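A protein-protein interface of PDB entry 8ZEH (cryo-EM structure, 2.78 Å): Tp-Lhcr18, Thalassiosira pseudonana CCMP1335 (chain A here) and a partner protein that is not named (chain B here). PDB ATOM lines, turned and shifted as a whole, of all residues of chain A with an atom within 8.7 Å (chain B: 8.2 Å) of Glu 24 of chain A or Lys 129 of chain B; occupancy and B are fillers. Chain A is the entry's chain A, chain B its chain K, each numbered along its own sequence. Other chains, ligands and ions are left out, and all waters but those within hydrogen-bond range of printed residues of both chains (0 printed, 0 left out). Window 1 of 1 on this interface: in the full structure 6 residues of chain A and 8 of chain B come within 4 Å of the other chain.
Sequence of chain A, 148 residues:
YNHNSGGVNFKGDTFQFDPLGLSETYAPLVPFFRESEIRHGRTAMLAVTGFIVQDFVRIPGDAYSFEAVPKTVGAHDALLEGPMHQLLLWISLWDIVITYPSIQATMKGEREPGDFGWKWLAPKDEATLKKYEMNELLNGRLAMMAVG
O of Leu 20 of chain A lies within hydrogen-bond range of NZ of Lys 130 of chain B, 3.2 Å away.
OE2 of Glu 24 of chain A lies within salt-bridge range of NZ of Lys 129 of chain B (3.6 Å).
The backbone carbonyl oxygen of Met 125 of chain B lies close to the backbone carbonyl oxygen of Leu 20 of chain A, at 3.5 Å.
O of Gly 21 of chain A is in hydrogen-bond range of OG1 of Thr 25 of chain A, 3.4 Å away.
The side-chain carboxylate (OD1) of Asp 123 of chain B lies within hydrogen-bond range of the backbone NH (N) of Gly 126 of chain B (3.3 Å).
The side-chain carboxylate (OD1) of Asp 123 of chain B sits at hydrogen-bond distance from the backbone NH (N) of Met 127 of chain B, at 3.1 Å.
The side-chain carboxylate (OD2) of Asp 123 of chain B is in hydrogen-bond range of the side-chain hydroxyl (OG1) of Thr 128 of chain B, at 2.7 Å.
The backbone carbonyl oxygen of Met 125 of chain B lies within hydrogen-bond range of the side-chain amino group of Lys 130 of chain B.
The backbone carbonyl oxygen (O) of Gly 126 of chain B sits close to the side-chain amino group (NZ) of Lys 130 of chain B (3.3 Å).
Among the printed residues, pairs that only touch across the chains: Thr 25 of chain A with Asp 123 of chain B and Leu 20 of chain A with Gly 126 of chain B.
Of chain B, only Lys 129 (3.3 Å) comes within 4 Å of Glu 24 of chain A.
Ala 27 of chain A touches none of the printed residues of chain B.
Printed residues of chain A within 4 Å of Asp 123 of chain B: Thr 25 (3.4 Å).
Printed residues of chain A within 4 Å of Gly 126 of chain B: Leu 20.
Lys 129 of chain B touches just one residue of chain A: Glu 24 (3.3 Å).
The nearest printed residue of chain A that does not touch Met 125 of chain B is Gly 21 of chain A (5.4 Å).
Printed residues of chain B that touch a printed residue of chain A: Asp 123, Met 125, Gly 126, Lys 129 and Lys 130.
Among the printed residues, Asp or Glu carboxylates within 4 Å of a Lys or Arg side-chain nitrogen of the other chain: Glu 24 of chain A with Lys 129 of chain B.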
ATOM      1  N   TYR A   1       9.317  -3.194 -34.154  1.00  0.00           N
ATOM      2  CA  TYR A   1       9.877  -4.367 -34.819  1.00  0.00           C
ATOM      3  C   TYR A   1       8.898  -4.938 -35.824  1.00  0.00           C
ATOM      4  O   TYR A   1       9.300  -5.502 -36.836  1.00  0.00           O
ATOM      5  CB  TYR A   1      10.258  -5.451 -33.812  1.00  0.00           C
ATOM      6  CG  TYR A   1      11.378  -5.070 -32.877  1.00  0.00           C
ATOM      7  CD1 TYR A   1      12.693  -5.055 -33.311  1.00  0.00           C
ATOM      8  CD2 TYR A   1      11.120  -4.743 -31.555  1.00  0.00           C
ATOM      9  CE1 TYR A   1      13.719  -4.712 -32.458  1.00  0.00           C
ATOM     10  CE2 TYR A   1      12.141  -4.399 -30.693  1.00  0.00           C
ATOM     11  CZ  TYR A   1      13.439  -4.386 -31.150  1.00  0.00           C
ATOM     12  OH  TYR A   1      14.460  -4.048 -30.296  1.00  0.00           O
ATOM     13  N   ASN A   2       7.611  -4.806 -35.542  1.00  0.00           N
ATOM     14  CA  ASN A   2       6.596  -5.295 -36.463  1.00  0.00           C
ATOM     15  C   ASN A   2       6.499  -4.410 -37.688  1.00  0.00           C
ATOM     16  O   ASN A   2       6.358  -4.903 -38.804  1.00  0.00           O
ATOM     17  CB  ASN A   2       5.241  -5.350 -35.769  1.00  0.00           C
ATOM     18  CG  ASN A   2       5.281  -6.149 -34.483  1.00  0.00           C
ATOM     19  OD1 ASN A   2       6.299  -6.751 -34.144  1.00  0.00           O
ATOM     20  ND2 ASN A   2       4.169  -6.157 -33.758  1.00  0.00           N
ATOM     21  N   HIS A   3       6.561  -3.102 -37.484  1.00  0.00           N
ATOM     22  CA  HIS A   3       6.440  -2.163 -38.592  1.00  0.00           C
ATOM     23  C   HIS A   3       7.633  -2.183 -39.528  1.00  0.00           C
ATOM     24  O   HIS A   3       7.465  -2.166 -40.744  1.00  0.00           O
ATOM     25  CB  HIS A   3       6.273  -0.751 -38.040  1.00  0.00           C
ATOM     26  CG  HIS A   3       7.479  -0.247 -37.313  1.00  0.00           C
ATOM     27  ND1 HIS A   3       8.107   0.935 -37.641  1.00  0.00           N
ATOM     28  CD2 HIS A   3       8.190  -0.779 -36.290  1.00  0.00           C
ATOM     29  CE1 HIS A   3       9.143   1.117 -36.841  1.00  0.00           C
ATOM     30  NE2 HIS A   3       9.216   0.090 -36.014  1.00  0.00           N
ATOM     31  N   GLN A  16      15.771  -8.943 -31.633  1.00  0.00           N
ATOM     32  CA  GLN A  16      15.241  -7.611 -31.409  1.00  0.00           C
ATOM     33  C   GLN A  16      16.192  -6.854 -30.513  1.00  0.00           C
ATOM     34  O   GLN A  16      16.456  -7.281 -29.394  1.00  0.00           O
ATOM     35  CB  GLN A  16      13.857  -7.695 -30.786  1.00  0.00           C
ATOM     36  CG  GLN A  16      12.819  -8.311 -31.707  1.00  0.00           C
ATOM     37  CD  GLN A  16      11.419  -8.244 -31.135  1.00  0.00           C
ATOM     38  OE1 GLN A  16      11.223  -7.833 -29.994  1.00  0.00           O
ATOM     39  NE2 GLN A  16      10.436  -8.650 -31.929  1.00  0.00           N
ATOM     40  N   ASP A  18      16.886  -3.200 -28.815  1.00  0.00           N
ATOM     41  CA  ASP A  18      16.623  -1.806 -28.486  1.00  0.00           C
ATOM     42  C   ASP A  18      16.691  -1.715 -26.982  1.00  0.00           C
ATOM     43  O   ASP A  18      15.681  -1.484 -26.323  1.00  0.00           O
ATOM     44  CB  ASP A  18      15.264  -1.346 -28.997  1.00  0.00           C
ATOM     45  CG  ASP A  18      15.039   0.142 -28.794  1.00  0.00           C
ATOM     46  OD1 ASP A  18      15.976   0.834 -28.344  1.00  0.00           O
ATOM     47  OD2 ASP A  18      13.924   0.623 -29.084  1.00  0.00           O
ATOM     48  N   LEU A  20      17.832   0.507 -24.910  1.00  0.00           N
ATOM     49  CA  LEU A  20      17.439   1.781 -24.324  1.00  0.00           C
ATOM     50  C   LEU A  20      15.949   2.047 -24.478  1.00  0.00           C
ATOM     51  O   LEU A  20      15.387   2.874 -23.766  1.00  0.00           O
ATOM     52  CB  LEU A  20      18.237   2.918 -24.955  1.00  0.00           C
ATOM     53  CG  LEU A  20      19.751   2.840 -24.778  1.00  0.00           C
ATOM     54  CD1 LEU A  20      20.416   4.030 -25.449  1.00  0.00           C
ATOM     55  CD2 LEU A  20      20.096   2.794 -23.299  1.00  0.00           C
ATOM     56  N   GLY A  21      15.306   1.349 -25.406  1.00  0.00           N
ATOM     57  CA  GLY A  21      13.885   1.548 -25.626  1.00  0.00           C
ATOM     58  C   GLY A  21      13.624   2.867 -26.309  1.00  0.00           C
ATOM     59  O   GLY A  21      12.556   3.451 -26.147  1.00  0.00           O
ATOM     60  N   LEU A  22      14.591   3.341 -27.084  1.00  0.00           N
ATOM     61  CA  LEU A  22      14.452   4.636 -27.738  1.00  0.00           C
ATOM     62  C   LEU A  22      13.237   4.685 -28.643  1.00  0.00           C
ATOM     63  O   LEU A  22      12.561   5.708 -28.720  1.00  0.00           O
ATOM     64  CB  LEU A  22      15.709   4.955 -28.547  1.00  0.00           C
ATOM     65  CG  LEU A  22      17.014   5.080 -27.760  1.00  0.00           C
ATOM     66  CD1 LEU A  22      18.182   5.318 -28.704  1.00  0.00           C
ATOM     67  CD2 LEU A  22      16.911   6.198 -26.735  1.00  0.00           C
ATOM     68  N   SER A  23      12.946   3.584 -29.322  1.00  0.00           N
ATOM     69  CA  SER A  23      11.832   3.568 -30.258  1.00  0.00           C
ATOM     70  C   SER A  23      10.534   3.955 -29.579  1.00  0.00           C
ATOM     71  O   SER A  23       9.771   4.749 -30.108  1.00  0.00           O
ATOM     72  CB  SER A  23      11.688   2.185 -30.878  1.00  0.00           C
ATOM     73  OG  SER A  23      12.900   1.777 -31.488  1.00  0.00           O
ATOM     74  N   GLU A  24      10.278   3.396 -28.406  1.00  0.00           N
ATOM     75  CA  GLU A  24       9.052   3.702 -27.683  1.00  0.00           C
ATOM     76  C   GLU A  24       9.041   5.130 -27.164  1.00  0.00           C
ATOM     77  O   GLU A  24       8.054   5.841 -27.322  1.00  0.00           O
ATOM     78  CB  GLU A  24       8.879   2.730 -26.521  1.00  0.00           C
ATOM     79  CG  GLU A  24       9.012   1.271 -26.920  1.00  0.00           C
ATOM     80  CD  GLU A  24       7.913   0.819 -27.862  1.00  0.00           C
ATOM     81  OE1 GLU A  24       8.093  -0.221 -28.528  1.00  0.00           O
ATOM     82  OE2 GLU A  24       6.871   1.504 -27.940  1.00  0.00           O
ATOM     83  N   THR A  25      10.140   5.555 -26.553  1.00  0.00           N
ATOM     84  CA  THR A  25      10.214   6.900 -26.002  1.00  0.00           C
ATOM     85  C   THR A  25      10.102   7.940 -27.098  1.00  0.00           C
ATOM     86  O   THR A  25       9.525   9.003 -26.890  1.00  0.00           O
ATOM     87  CB  THR A  25      11.524   7.126 -25.237  1.00  0.00           C
ATOM     88  OG1 THR A  25      12.633   6.869 -26.107  1.00  0.00           O
ATOM     89  CG2 THR A  25      11.607   6.193 -24.042  1.00  0.00           C
ATOM     90  N   TYR A  26      10.657   7.643 -28.265  1.00  0.00           N
ATOM     91  CA  TYR A  26      10.608   8.584 -29.370  1.00  0.00           C
ATOM     92  C   TYR A  26      10.071   7.902 -30.614  1.00  0.00           C
ATOM     93  O   TYR A  26      10.748   7.850 -31.638  1.00  0.00           O
ATOM     94  CB  TYR A  26      11.997   9.150 -29.631  1.00  0.00           C
ATOM     95  CG  TYR A  26      12.638   9.769 -28.414  1.00  0.00           C
ATOM     96  CD1 TYR A  26      12.158  10.957 -27.882  1.00  0.00           C
ATOM     97  CD2 TYR A  26      13.726   9.169 -27.797  1.00  0.00           C
ATOM     98  CE1 TYR A  26      12.741  11.527 -26.768  1.00  0.00           C
ATOM     99  CE2 TYR A  26      14.316   9.733 -26.683  1.00  0.00           C
ATOM    100  CZ  TYR A  26      13.819  10.913 -26.174  1.00  0.00           C
ATOM    101  OH  TYR A  26      14.402  11.480 -25.065  1.00  0.00           O
ATOM    102  N   ALA A  27       8.853   7.386 -30.536  1.00  0.00           N
ATOM    103  CA  ALA A  27       8.277   6.657 -31.663  1.00  0.00           C
ATOM    104  C   ALA A  27       8.044   7.500 -32.910  1.00  0.00           C
ATOM    105  O   ALA A  27       8.389   7.081 -34.011  1.00  0.00           O
ATOM    106  CB  ALA A  27       6.978   5.991 -31.237  1.00  0.00           C
ATOM    107  N   PRO A  28       7.424   8.683 -32.757  1.00  0.00           N
ATOM    108  CA  PRO A  28       7.119   9.429 -33.982  1.00  0.00           C
ATOM    109  C   PRO A  28       8.351   9.731 -34.819  1.00  0.00           C
ATOM    110  O   PRO A  28       8.200  10.165 -35.956  1.00  0.00           O
ATOM    111  CB  PRO A  28       6.532  10.739 -33.456  1.00  0.00           C
ATOM    112  CG  PRO A  28       6.010  10.411 -32.103  1.00  0.00           C
ATOM    113  CD  PRO A  28       6.981   9.415 -31.553  1.00  0.00           C
ATOM    114  N   LEU A  29       9.545   9.516 -34.280  1.00  0.00           N
ATOM    115  CA  LEU A  29      10.760   9.866 -35.007  1.00  0.00           C
ATOM    116  C   LEU A  29      11.455   8.658 -35.613  1.00  0.00           C
ATOM    117  O   LEU A  29      12.504   8.795 -36.235  1.00  0.00           O
ATOM    118  CB  LEU A  29      11.730  10.602 -34.085  1.00  0.00           C
ATOM    119  CG  LEU A  29      11.244  11.917 -33.481  1.00  0.00           C
ATOM    120  CD1 LEU A  29      12.309  12.490 -32.559  1.00  0.00           C
ATOM    121  CD2 LEU A  29      10.894  12.905 -34.581  1.00  0.00           C
ATOM    122  N   VAL A  30      10.875   7.478 -35.448  1.00  0.00           N
ATOM    123  CA  VAL A  30      11.510   6.260 -35.952  1.00  0.00           C
ATOM    124  C   VAL A  30      11.777   6.305 -37.457  1.00  0.00           C
ATOM    125  O   VAL A  30      12.805   5.813 -37.914  1.00  0.00           O
ATOM    126  CB  VAL A  30      10.678   5.009 -35.617  1.00  0.00           C
ATOM    127  CG1 VAL A  30      11.291   3.776 -36.261  1.00  0.00           C
ATOM    128  CG2 VAL A  30      10.584   4.835 -34.110  1.00  0.00           C
ATOM    129  N   PHE A  33      14.980   7.822 -37.860  1.00  0.00           N
ATOM    130  CA  PHE A  33      16.021   6.928 -37.393  1.00  0.00           C
ATOM    131  C   PHE A  33      16.375   5.931 -38.479  1.00  0.00           C
ATOM    132  O   PHE A  33      17.550   5.679 -38.731  1.00  0.00           O
ATOM    133  CB  PHE A  33      15.571   6.196 -36.136  1.00  0.00           C
ATOM    134  CG  PHE A  33      15.265   7.103 -34.981  1.00  0.00           C
ATOM    135  CD1 PHE A  33      16.010   8.248 -34.769  1.00  0.00           C
ATOM    136  CD2 PHE A  33      14.243   6.803 -34.099  1.00  0.00           C
ATOM    137  CE1 PHE A  33      15.734   9.085 -33.705  1.00  0.00           C
ATOM    138  CE2 PHE A  33      13.961   7.634 -33.032  1.00  0.00           C
ATOM    139  CZ  PHE A  33      14.709   8.776 -32.835  1.00  0.00           C
ATOM    140  N   ASP B 123      13.599  10.871 -20.849  1.00  0.00           N
ATOM    141  CA  ASP B 123      13.763   9.539 -20.285  1.00  0.00           C
ATOM    142  C   ASP B 123      14.336   8.646 -21.363  1.00  0.00           C
ATOM    143  O   ASP B 123      13.650   7.764 -21.874  1.00  0.00           O
ATOM    144  CB  ASP B 123      12.440   8.974 -19.787  1.00  0.00           C
ATOM    145  CG  ASP B 123      12.585   7.575 -19.215  1.00  0.00           C
ATOM    146  OD1 ASP B 123      13.667   7.260 -18.677  1.00  0.00           O
ATOM    147  OD2 ASP B 123      11.621   6.790 -19.302  1.00  0.00           O
ATOM    148  N   MET B 125      16.602   6.370 -21.134  1.00  0.00           N
ATOM    149  CA  MET B 125      16.844   5.002 -20.686  1.00  0.00           C
ATOM    150  C   MET B 125      15.553   4.207 -20.596  1.00  0.00           C
ATOM    151  O   MET B 125      15.577   3.019 -20.297  1.00  0.00           O
ATOM    152  CB  MET B 125      17.557   5.004 -19.338  1.00  0.00           C
ATOM    153  CG  MET B 125      18.909   5.693 -19.361  1.00  0.00           C
ATOM    154  SD  MET B 125      19.658   5.770 -17.726  1.00  0.00           S
ATOM    155  CE  MET B 125      18.400   6.678 -16.834  1.00  0.00           C
ATOM    156  N   GLY B 126      14.424   4.859 -20.841  1.00  0.00           N
ATOM    157  CA  GLY B 126      13.148   4.167 -20.830  1.00  0.00           C
ATOM    158  C   GLY B 126      12.744   3.612 -19.483  1.00  0.00           C
ATOM    159  O   GLY B 126      11.966   2.665 -19.409  1.00  0.00           O
ATOM    160  N   MET B 127      13.251   4.206 -18.412  1.00  0.00           N
ATOM    161  CA  MET B 127      12.942   3.720 -17.076  1.00  0.00           C
ATOM    162  C   MET B 127      11.448   3.749 -16.813  1.00  0.00           C
ATOM    163  O   MET B 127      10.929   2.918 -16.076  1.00  0.00           O
ATOM    164  CB  MET B 127      13.665   4.556 -16.027  1.00  0.00           C
ATOM    165  CG  MET B 127      15.177   4.501 -16.142  1.00  0.00           C
ATOM    166  SD  MET B 127      15.787   2.810 -16.046  1.00  0.00           S
ATOM    167  CE  MET B 127      17.549   3.077 -16.217  1.00  0.00           C
ATOM    168  N   THR B 128      10.749   4.697 -17.423  1.00  0.00           N
ATOM    169  CA  THR B 128       9.315   4.825 -17.190  1.00  0.00           C
ATOM    170  C   THR B 128       8.566   3.565 -17.591  1.00  0.00           C
ATOM    171  O   THR B 128       7.449   3.337 -17.135  1.00  0.00           O
ATOM    172  CB  THR B 128       8.724   6.017 -17.958  1.00  0.00           C
ATOM    173  OG1 THR B 128       9.077   5.917 -19.341  1.00  0.00           O
ATOM    174  CG2 THR B 128       9.259   7.323 -17.395  1.00  0.00           C
ATOM    175  N   LYS B 129       9.165   2.754 -18.452  1.00  0.00           N
ATOM    176  CA  LYS B 129       8.537   1.500 -18.844  1.00  0.00           C
ATOM    177  C   LYS B 129       9.273   0.326 -18.223  1.00  0.00           C
ATOM    178  O   LYS B 129       8.749  -0.784 -18.165  1.00  0.00           O
ATOM    179  CB  LYS B 129       8.520   1.367 -20.364  1.00  0.00           C
ATOM    180  CG  LYS B 129       7.837   0.109 -20.873  1.00  0.00           C
ATOM    181  CD  LYS B 129       7.759   0.096 -22.389  1.00  0.00           C
ATOM    182  CE  LYS B 129       6.938   1.267 -22.904  1.00  0.00           C
ATOM    183  NZ  LYS B 129       6.791   1.232 -24.385  1.00  0.00           N
ATOM    184  N   LYS B 130      10.484   0.570 -17.742  1.00  0.00           N
ATOM    185  CA  LYS B 130      11.280  -0.503 -17.168  1.00  0.00           C
ATOM    186  C   LYS B 130      11.175  -0.563 -15.648  1.00  0.00           C
ATOM    187  O   LYS B 130      11.822  -1.400 -15.020  1.00  0.00           O
ATOM    188  CB  LYS B 130      12.741  -0.336 -17.577  1.00  0.00           C
ATOM    189  CG  LYS B 130      12.964  -0.286 -19.078  1.00  0.00           C
ATOM    190  CD  LYS B 130      14.417   0.012 -19.406  1.00  0.00           C
ATOM    191  CE  LYS B 130      14.650   0.032 -20.907  1.00  0.00           C
ATOM    192  NZ  LYS B 130      13.822   1.064 -21.586  1.00  0.00           N
ATOM    193  N   LEU B 131      10.371   0.310 -15.050  1.00  0.00           N
ATOM    194  CA  LEU B 131      10.259   0.346 -13.593  1.00  0.00           C
ATOM    195  C   LEU B 131       8.815   0.326 -13.126  1.00  0.00           C
ATOM    196  O   LEU B 131       7.913   0.675 -13.883  1.00  0.00           O
ATOM    197  CB  LEU B 131      10.954   1.584 -13.027  1.00  0.00           C
ATOM    198  CG  LEU B 131      12.426   1.801 -13.369  1.00  0.00           C
ATOM    199  CD1 LEU B 131      12.911   3.119 -12.784  1.00  0.00           C
ATOM    200  CD2 LEU B 131      13.268   0.643 -12.858  1.00  0.00           C
ATOM    201  N   SER B 132       8.594  -0.078 -11.880  1.00  0.00           N
ATOM    202  CA  SER B 132       7.242  -0.119 -11.328  1.00  0.00           C
ATOM    203  C   SER B 132       6.784   1.252 -10.868  1.00  0.00           C
ATOM    204  O   SER B 132       7.604   2.083 -10.481  1.00  0.00           O
ATOM    205  CB  SER B 132       7.183  -1.103 -10.166  1.00  0.00           C
ATOM    206  OG  SER B 132       8.213  -0.840  -9.231  1.00  0.00           O
ATOM    207  N   LEU B 136       8.981   4.656  -9.664  1.00  0.00           N
ATOM    208  CA  LEU B 136       9.017   5.925 -10.368  1.00  0.00           C
ATOM    209  C   LEU B 136       8.673   7.068  -9.434  1.00  0.00           C
ATOM    210  O   LEU B 136       9.404   8.052  -9.362  1.00  0.00           O
ATOM    211  CB  LEU B 136       8.052   5.922 -11.551  1.00  0.00           C
ATOM    212  CG  LEU B 136       8.538   5.284 -12.852  1.00  0.00           C
ATOM    213  CD1 LEU B 136       9.992   5.645 -13.108  1.00  0.00           C
ATOM    214  CD2 LEU B 136       8.361   3.776 -12.823  1.00  0.00           C
